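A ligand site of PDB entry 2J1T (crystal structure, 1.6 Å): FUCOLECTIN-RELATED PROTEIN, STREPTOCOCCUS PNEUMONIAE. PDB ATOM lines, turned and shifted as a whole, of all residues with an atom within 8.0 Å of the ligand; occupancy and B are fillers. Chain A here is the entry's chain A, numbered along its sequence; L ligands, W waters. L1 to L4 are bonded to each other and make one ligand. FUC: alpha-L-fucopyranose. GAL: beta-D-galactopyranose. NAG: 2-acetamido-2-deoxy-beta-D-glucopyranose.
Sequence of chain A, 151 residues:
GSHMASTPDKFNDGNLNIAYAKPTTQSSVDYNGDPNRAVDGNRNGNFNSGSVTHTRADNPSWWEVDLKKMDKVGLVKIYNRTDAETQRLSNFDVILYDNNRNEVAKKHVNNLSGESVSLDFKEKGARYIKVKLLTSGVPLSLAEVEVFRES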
ATOM      1  N   ASP A  30     -17.232 -19.110 -36.546  1.00  0.00           N
ATOM      2  CA  ASP A  30     -16.926 -17.956 -35.700  1.00  0.00           C
ATOM      3  C   ASP A  30     -16.182 -18.456 -34.470  1.00  0.00           C
ATOM      4  O   ASP A  30     -16.320 -19.625 -34.057  1.00  0.00           O
ATOM      5  CB  ASP A  30     -18.226 -17.171 -35.377  1.00  0.00           C
ATOM      6  CG  ASP A  30     -17.961 -15.697 -35.090  1.00  0.00           C
ATOM      7  OD1 ASP A  30     -16.771 -15.244 -35.202  1.00  0.00           O
ATOM      8  OD2 ASP A  30     -18.909 -14.927 -34.836  1.00  0.00           O
ATOM      9  N   TYR A  31     -15.336 -17.605 -33.892  1.00  0.00           N
ATOM     10  CA  TYR A  31     -14.609 -17.892 -32.664  1.00  0.00           C
ATOM     11  C   TYR A  31     -13.755 -19.154 -32.756  1.00  0.00           C
ATOM     12  O   TYR A  31     -13.569 -19.836 -31.768  1.00  0.00           O
ATOM     13  CB  TYR A  31     -15.520 -17.953 -31.450  1.00  0.00           C
ATOM     14  CG  TYR A  31     -16.329 -16.675 -31.216  1.00  0.00           C
ATOM     15  CD1 TYR A  31     -17.656 -16.620 -31.559  1.00  0.00           C
ATOM     16  CD2 TYR A  31     -15.745 -15.547 -30.663  1.00  0.00           C
ATOM     17  CE1 TYR A  31     -18.422 -15.473 -31.363  1.00  0.00           C
ATOM     18  CE2 TYR A  31     -16.483 -14.401 -30.450  1.00  0.00           C
ATOM     19  CZ  TYR A  31     -17.840 -14.386 -30.802  1.00  0.00           C
ATOM     20  OH  TYR A  31     -18.607 -13.240 -30.623  1.00  0.00           O
ATOM     21  N   ASN A  32     -13.309 -19.468 -33.981  1.00  0.00           N
ATOM     22  CA  ASN A  32     -12.496 -20.652 -34.274  1.00  0.00           C
ATOM     23  C   ASN A  32     -13.223 -21.937 -33.956  1.00  0.00           C
ATOM     24  O   ASN A  32     -12.582 -23.009 -33.819  1.00  0.00           O
ATOM     25  CB  ASN A  32     -11.135 -20.572 -33.559  1.00  0.00           C
ATOM     26  CG  ASN A  32     -10.356 -19.351 -33.931  1.00  0.00           C
ATOM     27  OD1 ASN A  32     -10.334 -18.978 -35.086  1.00  0.00           O
ATOM     28  ND2 ASN A  32      -9.693 -18.746 -32.949  1.00  0.00           N
ATOM     29  N   ASN A  46     -17.975 -26.947 -22.578  1.00  0.00           N
ATOM     30  CA  ASN A  46     -17.484 -25.602 -22.275  1.00  0.00           C
ATOM     31  C   ASN A  46     -16.796 -25.068 -23.512  1.00  0.00           C
ATOM     32  O   ASN A  46     -15.819 -25.613 -23.985  1.00  0.00           O
ATOM     33  CB  ASN A  46     -16.607 -25.595 -21.025  1.00  0.00           C
ATOM     34  CG  ASN A  46     -16.254 -24.242 -20.587  1.00  0.00           C
ATOM     35  OD1 ASN A  46     -16.141 -23.302 -21.413  1.00  0.00           O
ATOM     36  ND2 ASN A  46     -16.019 -24.083 -19.254  1.00  0.00           N
ATOM     37  N   PHE A  47     -17.336 -23.985 -24.063  1.00  0.00           N
ATOM     38  CA  PHE A  47     -16.805 -23.468 -25.295  1.00  0.00           C
ATOM     39  C   PHE A  47     -15.315 -23.165 -25.172  1.00  0.00           C
ATOM     40  O   PHE A  47     -14.546 -23.344 -26.112  1.00  0.00           O
ATOM     41  CB  PHE A  47     -17.569 -22.201 -25.779  1.00  0.00           C
ATOM     42  CG  PHE A  47     -17.107 -21.757 -27.116  1.00  0.00           C
ATOM     43  CD1 PHE A  47     -16.220 -20.728 -27.239  1.00  0.00           C
ATOM     44  CD2 PHE A  47     -17.459 -22.476 -28.269  1.00  0.00           C
ATOM     45  CE1 PHE A  47     -15.719 -20.378 -28.483  1.00  0.00           C
ATOM     46  CE2 PHE A  47     -16.915 -22.110 -29.503  1.00  0.00           C
ATOM     47  CZ  PHE A  47     -16.034 -21.067 -29.592  1.00  0.00           C
ATOM     48  N   ASN A  48     -14.892 -22.744 -23.999  1.00  0.00           N
ATOM     49  CA  ASN A  48     -13.470 -22.402 -23.836  1.00  0.00           C
ATOM     50  C   ASN A  48     -12.488 -23.567 -23.792  1.00  0.00           C
ATOM     51  O   ASN A  48     -11.238 -23.337 -23.872  1.00  0.00           O
ATOM     52  CB  ASN A  48     -13.290 -21.462 -22.683  1.00  0.00           C
ATOM     53  CG  ASN A  48     -13.811 -20.077 -23.001  1.00  0.00           C
ATOM     54  OD1 ASN A  48     -13.726 -19.578 -24.177  1.00  0.00           O
ATOM     55  ND2 ASN A  48     -14.379 -19.441 -22.003  1.00  0.00           N
ATOM     56  N   THR A  53     -18.219 -26.506 -31.413  1.00  0.00           N
ATOM     57  CA  THR A  53     -18.299 -25.754 -32.662  1.00  0.00           C
ATOM     58  C   THR A  53     -18.978 -24.417 -32.441  1.00  0.00           C
ATOM     59  O   THR A  53     -19.550 -24.163 -31.394  1.00  0.00           O
ATOM     60  CB  THR A  53     -19.064 -26.535 -33.710  1.00  0.00           C
ATOM     61  OG1 THR A  53     -20.457 -26.599 -33.349  1.00  0.00           O
ATOM     62  CG2 THR A  53     -18.548 -28.007 -33.885  1.00  0.00           C
ATOM     63  N   HIS A  54     -18.923 -23.583 -33.472  1.00  0.00           N
ATOM     64  CA  HIS A  54     -19.584 -22.267 -33.469  1.00  0.00           C
ATOM     65  C   HIS A  54     -19.642 -21.711 -34.878  1.00  0.00           C
ATOM     66  O   HIS A  54     -18.628 -21.494 -35.550  1.00  0.00           O
ATOM     67  CB  HIS A  54     -18.785 -21.320 -32.601  1.00  0.00           C
ATOM     68  CG  HIS A  54     -19.575 -20.208 -31.980  1.00  0.00           C
ATOM     69  ND1 HIS A  54     -20.157 -19.181 -32.705  1.00  0.00           N
ATOM     70  CD2 HIS A  54     -19.773 -19.913 -30.671  1.00  0.00           C
ATOM     71  CE1 HIS A  54     -20.723 -18.331 -31.868  1.00  0.00           C
ATOM     72  NE2 HIS A  54     -20.498 -18.738 -30.622  1.00  0.00           N
ATOM     73  N   THR A  55     -20.847 -21.474 -35.340  1.00  0.00           N
ATOM     74  CA  THR A  55     -21.016 -20.770 -36.636  1.00  0.00           C
ATOM     75  C   THR A  55     -21.253 -19.276 -36.370  1.00  0.00           C
ATOM     76  O   THR A  55     -21.440 -18.859 -35.226  1.00  0.00           O
ATOM     77  CB  THR A  55     -22.226 -21.327 -37.448  1.00  0.00           C
ATOM     78  OG1 THR A  55     -23.459 -21.003 -36.758  1.00  0.00           O
ATOM     79  CG2 THR A  55     -22.255 -22.828 -37.541  1.00  0.00           C
ATOM     80  N   ARG A  81     -23.541 -27.229 -26.161  1.00  0.00           N
ATOM     81  CA  ARG A  81     -22.815 -26.283 -25.360  1.00  0.00           C
ATOM     82  C   ARG A  81     -23.426 -26.226 -23.929  1.00  0.00           C
ATOM     83  O   ARG A  81     -24.626 -26.329 -23.754  1.00  0.00           O
ATOM     84  CB  ARG A  81     -22.852 -24.887 -26.035  1.00  0.00           C
ATOM     85  CG  ARG A  81     -21.870 -23.884 -25.412  1.00  0.00           C
ATOM     86  CD  ARG A  81     -21.853 -22.543 -26.020  1.00  0.00           C
ATOM     87  NE  ARG A  81     -21.008 -21.628 -25.278  1.00  0.00           N
ATOM     88  CZ  ARG A  81     -20.815 -20.386 -25.605  1.00  0.00           C
ATOM     89  NH1 ARG A  81     -21.400 -19.881 -26.647  1.00  0.00           N
ATOM     90  NH2 ARG A  81     -20.013 -19.606 -24.887  1.00  0.00           N
ATOM     91  N   ASP A  83     -21.546 -24.125 -21.135  1.00  0.00           N
ATOM     92  CA  ASP A  83     -21.071 -23.003 -20.290  1.00  0.00           C
ATOM     93  C   ASP A  83     -21.944 -21.763 -20.411  1.00  0.00           C
ATOM     94  O   ASP A  83     -22.014 -20.938 -19.448  1.00  0.00           O
ATOM     95  CB  ASP A  83     -19.646 -22.585 -20.601  1.00  0.00           C
ATOM     96  CG  ASP A  83     -19.491 -22.040 -22.014  1.00  0.00           C
ATOM     97  OD1 ASP A  83     -19.177 -20.832 -22.202  1.00  0.00           O
ATOM     98  OD2 ASP A  83     -19.722 -22.782 -22.989  1.00  0.00           O
ATOM     99  N   ALA A  84     -22.547 -21.553 -21.584  1.00  0.00           N
ATOM    100  CA  ALA A  84     -23.375 -20.369 -21.829  1.00  0.00           C
ATOM    101  C   ALA A  84     -24.293 -20.633 -23.037  1.00  0.00           C
ATOM    102  O   ALA A  84     -24.039 -21.520 -23.820  1.00  0.00           O
ATOM    103  CB  ALA A  84     -22.532 -19.173 -22.108  1.00  0.00           C
ATOM    104  N   GLU A  85     -25.314 -19.797 -23.191  1.00  0.00           N
ATOM    105  CA  GLU A  85     -26.130 -19.723 -24.408  1.00  0.00           C
ATOM    106  C   GLU A  85     -26.751 -21.081 -24.771  1.00  0.00           C
ATOM    107  O   GLU A  85     -26.885 -21.418 -25.920  1.00  0.00           O
ATOM    108  CB  GLU A  85     -25.339 -19.139 -25.563  1.00  0.00           C
ATOM    109  CG  GLU A  85     -24.712 -17.767 -25.300  1.00  0.00           C
ATOM    110  CD  GLU A  85     -25.700 -16.622 -25.233  1.00  0.00           C
ATOM    111  OE1 GLU A  85     -26.944 -16.841 -25.269  1.00  0.00           O
ATOM    112  OE2 GLU A  85     -25.228 -15.460 -25.149  1.00  0.00           O
ATOM    113  N   GLN A  87     -29.667 -22.183 -24.690  1.00  0.00           N
ATOM    114  CA  GLN A  87     -30.935 -22.123 -25.335  1.00  0.00           C
ATOM    115  C   GLN A  87     -30.827 -22.054 -26.847  1.00  0.00           C
ATOM    116  O   GLN A  87     -31.828 -22.291 -27.552  1.00  0.00           O
ATOM    117  CB  GLN A  87     -31.706 -20.898 -24.844  1.00  0.00           C
ATOM    118  CG  GLN A  87     -31.300 -19.562 -25.425  1.00  0.00           C
ATOM    119  CD  GLN A  87     -29.937 -19.070 -25.022  1.00  0.00           C
ATOM    120  OE1 GLN A  87     -29.435 -19.424 -23.931  1.00  0.00           O
ATOM    121  NE2 GLN A  87     -29.361 -18.226 -25.833  1.00  0.00           N
ATOM    122  N   ARG A  88     -29.624 -21.763 -27.371  1.00  0.00           N
ATOM    123  CA  ARG A  88     -29.484 -21.634 -28.830  1.00  0.00           C
ATOM    124  C   ARG A  88     -29.790 -22.969 -29.496  1.00  0.00           C
ATOM    125  O   ARG A  88     -30.297 -22.985 -30.613  1.00  0.00           O
ATOM    126  CB  ARG A  88     -28.088 -21.205 -29.234  1.00  0.00           C
ATOM    127  CG  ARG A  88     -27.816 -19.753 -28.853  1.00  0.00           C
ATOM    128  CD  ARG A  88     -26.363 -19.359 -29.146  1.00  0.00           C
ATOM    129  NE  ARG A  88     -26.222 -17.910 -29.000  1.00  0.00           N
ATOM    130  CZ  ARG A  88     -25.070 -17.283 -28.933  1.00  0.00           C
ATOM    131  NH1 ARG A  88     -23.910 -17.966 -29.024  1.00  0.00           N
ATOM    132  NH2 ARG A  88     -25.049 -15.958 -28.782  1.00  0.00           N
ATOM    133  N   PRO A 139     -26.258 -18.401 -33.741  1.00  0.00           N
ATOM    134  CA  PRO A 139     -25.135 -19.349 -33.952  1.00  0.00           C
ATOM    135  C   PRO A 139     -25.470 -20.774 -33.482  1.00  0.00           C
ATOM    136  O   PRO A 139     -26.101 -20.958 -32.461  1.00  0.00           O
ATOM    137  CB  PRO A 139     -24.031 -18.795 -33.085  1.00  0.00           C
ATOM    138  CG  PRO A 139     -24.433 -17.340 -32.854  1.00  0.00           C
ATOM    139  CD  PRO A 139     -25.920 -17.357 -32.755  1.00  0.00           C
ATOM    140  N   SER A 141     -23.820 -24.101 -32.051  1.00  0.00           N
ATOM    141  CA  SER A 141     -22.697 -24.643 -31.328  1.00  0.00           C
ATOM    142  C   SER A 141     -23.042 -26.014 -30.793  1.00  0.00           C
ATOM    143  O   SER A 141     -24.003 -26.193 -30.056  1.00  0.00           O
ATOM    144  CB  SER A 141     -22.335 -23.751 -30.153  1.00  0.00           C
ATOM    145  OG  SER A 141     -21.725 -22.515 -30.551  1.00  0.00           O
HETATM  146  C1  FUC L   1     -20.887 -15.823 -25.335  1.00  0.00           C
HETATM  147  C2  FUC L   1     -21.947 -15.565 -26.444  1.00  0.00           C
HETATM  148  C3  FUC L   1     -21.320 -15.212 -27.800  1.00  0.00           C
HETATM  149  C4  FUC L   1     -20.319 -16.305 -28.166  1.00  0.00           C
HETATM  150  C5  FUC L   1     -19.295 -16.428 -27.026  1.00  0.00           C
HETATM  151  C6  FUC L   1     -18.227 -17.452 -27.358  1.00  0.00           C
HETATM  152  O2  FUC L   1     -22.880 -14.542 -26.086  1.00  0.00           O
HETATM  153  O3  FUC L   1     -22.285 -15.090 -28.791  1.00  0.00           O
HETATM  154  O4  FUC L   1     -21.021 -17.524 -28.288  1.00  0.00           O
HETATM  155  O5  FUC L   1     -19.872 -16.743 -25.737  1.00  0.00           O
HETATM  156  C1  GAL L   2     -18.349 -13.532 -24.096  1.00  0.00           C
HETATM  157  C2  GAL L   2     -19.648 -14.329 -23.888  1.00  0.00           C
HETATM  158  C3  GAL L   2     -20.576 -13.512 -23.018  1.00  0.00           C
HETATM  159  C4  GAL L   2     -19.778 -13.124 -21.752  1.00  0.00           C
HETATM  160  C5  GAL L   2     -18.452 -12.437 -22.051  1.00  0.00           C
HETATM  161  C6  GAL L   2     -17.594 -12.099 -20.823  1.00  0.00           C
HETATM  162  O2  GAL L   2     -20.288 -14.549 -25.140  1.00  0.00           O
HETATM  163  O3  GAL L   2     -21.666 -14.310 -22.617  1.00  0.00           O
HETATM  164  O4  GAL L   2     -19.502 -14.308 -21.027  1.00  0.00           O
HETATM  165  O5  GAL L   2     -17.651 -13.268 -22.866  1.00  0.00           O
HETATM  166  O6  GAL L   2     -16.579 -11.231 -21.274  1.00  0.00           O
HETATM  167  C1  NAG L   3     -14.352 -13.548 -27.402  1.00  0.00           C
HETATM  168  C2  NAG L   3     -14.010 -13.820 -25.948  1.00  0.00           C
HETATM  169  C3  NAG L   3     -15.196 -14.493 -25.300  1.00  0.00           C
HETATM  170  C4  NAG L   3     -16.444 -13.642 -25.514  1.00  0.00           C
HETATM  171  C5  NAG L   3     -16.656 -13.313 -26.997  1.00  0.00           C
HETATM  172  C6  NAG L   3     -17.808 -12.354 -27.285  1.00  0.00           C
HETATM  173  C7  NAG L   3     -11.638 -14.116 -25.429  1.00  0.00           C
HETATM  174  C8  NAG L   3     -10.483 -14.707 -26.192  1.00  0.00           C
HETATM  175  N2  NAG L   3     -12.817 -14.630 -25.776  1.00  0.00           N
HETATM  176  O1  NAG L   3     -13.349 -12.842 -28.066  1.00  0.00           O
HETATM  177  O3  NAG L   3     -14.957 -14.543 -23.912  1.00  0.00           O
HETATM  178  O4  NAG L   3     -17.532 -14.309 -24.943  1.00  0.00           O
HETATM  179  O5  NAG L   3     -15.469 -12.689 -27.411  1.00  0.00           O
HETATM  180  O6  NAG L   3     -17.549 -11.095 -26.682  1.00  0.00           O
HETATM  181  O7  NAG L   3     -11.487 -13.247 -24.561  1.00  0.00           O
HETATM  182  C1  FUC L   4     -14.464 -15.912 -23.213  1.00  0.00           C
HETATM  183  C2  FUC L   4     -14.167 -15.830 -21.719  1.00  0.00           C
HETATM  184  C3  FUC L   4     -15.456 -15.507 -20.964  1.00  0.00           C
HETATM  185  C4  FUC L   4     -16.527 -16.545 -21.288  1.00  0.00           C
HETATM  186  C5  FUC L   4     -16.740 -16.641 -22.806  1.00  0.00           C
HETATM  187  C6  FUC L   4     -17.669 -17.771 -23.225  1.00  0.00           C
HETATM  188  O2  FUC L   4     -13.227 -14.780 -21.671  1.00  0.00           O
HETATM  189  O3  FUC L   4     -15.290 -15.465 -19.547  1.00  0.00           O
HETATM  190  O4  FUC L   4     -16.072 -17.777 -20.755  1.00  0.00           O
HETATM  191  O5  FUC L   4     -15.513 -16.801 -23.496  1.00  0.00           O
HETATM  192  O   HOH W   1     -22.433 -11.844 -26.328  1.00  0.00           O
HETATM  193  O   HOH W   2      -9.919 -12.078 -21.899  1.00  0.00           O
HETATM  194  O   HOH W   3     -13.720 -17.371 -27.404  1.00  0.00           O
HETATM  195  O   HOH W   4     -21.433 -13.578 -30.921  1.00  0.00           O
HETATM  196  O   HOH W   5     -14.242 -12.222 -22.500  1.00  0.00           O
HETATM  197  O   HOH W   6     -18.325 -19.324 -20.257  1.00  0.00           O
HETATM  198  O   HOH W   7     -18.467 -15.604 -18.034  1.00  0.00           O
HETATM  199  O   HOH W   8     -17.427  -8.518 -21.063  1.00  0.00           O
HETATM  200  O   HOH W   9     -22.162 -15.886 -20.206  1.00  0.00           O
HETATM  201  O   HOH W  10     -14.361 -13.206 -18.343  1.00  0.00           O
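O4 of FUC L4 is in hydrogen-bond range of ND2 of Asn 48, at 2.7 Å. O4 of FUC L1 sits at hydrogen-bond distance from NE2 of His 54 (2.7 Å). The side-chain carboxylate (OE2) of Glu 85 sits at hydrogen-bond distance from an oxygen (O2) of FUC L1 (2.7 Å). O4 of FUC L1 lies within hydrogen-bond range of NH1 of Arg 81, 2.9 Å away. O3 of FUC L1 is in hydrogen-bond range of NH2 of Arg 88 (2.9 Å).
OD1 of Asn 46 lies within hydrogen-bond range of N of Asn 48. The backbone carbonyl oxygen of His 54 sits at hydrogen-bond distance from the backbone NH of Asp 30 (2.9 Å). OE2 of Glu 85 lies within salt-bridge range of NH2 of Arg 88 (3.7 Å). The side-chain amide nitrogen of Gln 87 lies within hydrogen-bond range of the side-chain carboxylate of Glu 85 (2.8 Å). NE of Arg 81 lies within salt-bridge range of OD2 of Asp 83 (2.9 Å). The guanidinium group of Arg 81 sits close to the backbone carbonyl oxygen of Ala 84. The side-chain carboxylate of Asp 83 is in hydrogen-bond range of the backbone NH of Phe 47, at 2.9 Å.
OH of Tyr 31 touches C6 of NAG L3, at 3.5 Å. CD1 of Phe 47 touches C6 of FUC L1, at 3.8 Å. OD1 of Asp 83 touches C6 of FUC L4, 3.6 Å away.
Water W4 bridges an oxygen (O3) of FUC L1 (2.7 Å) and the side-chain hydroxyl (OH) of Tyr 31 (2.9 Å). Water W6 lies within hydrogen-bond range of the side-chain carboxylate of Asp 83 (2.6 Å) and an oxygen (O4) of FUC L4 (2.8 Å).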
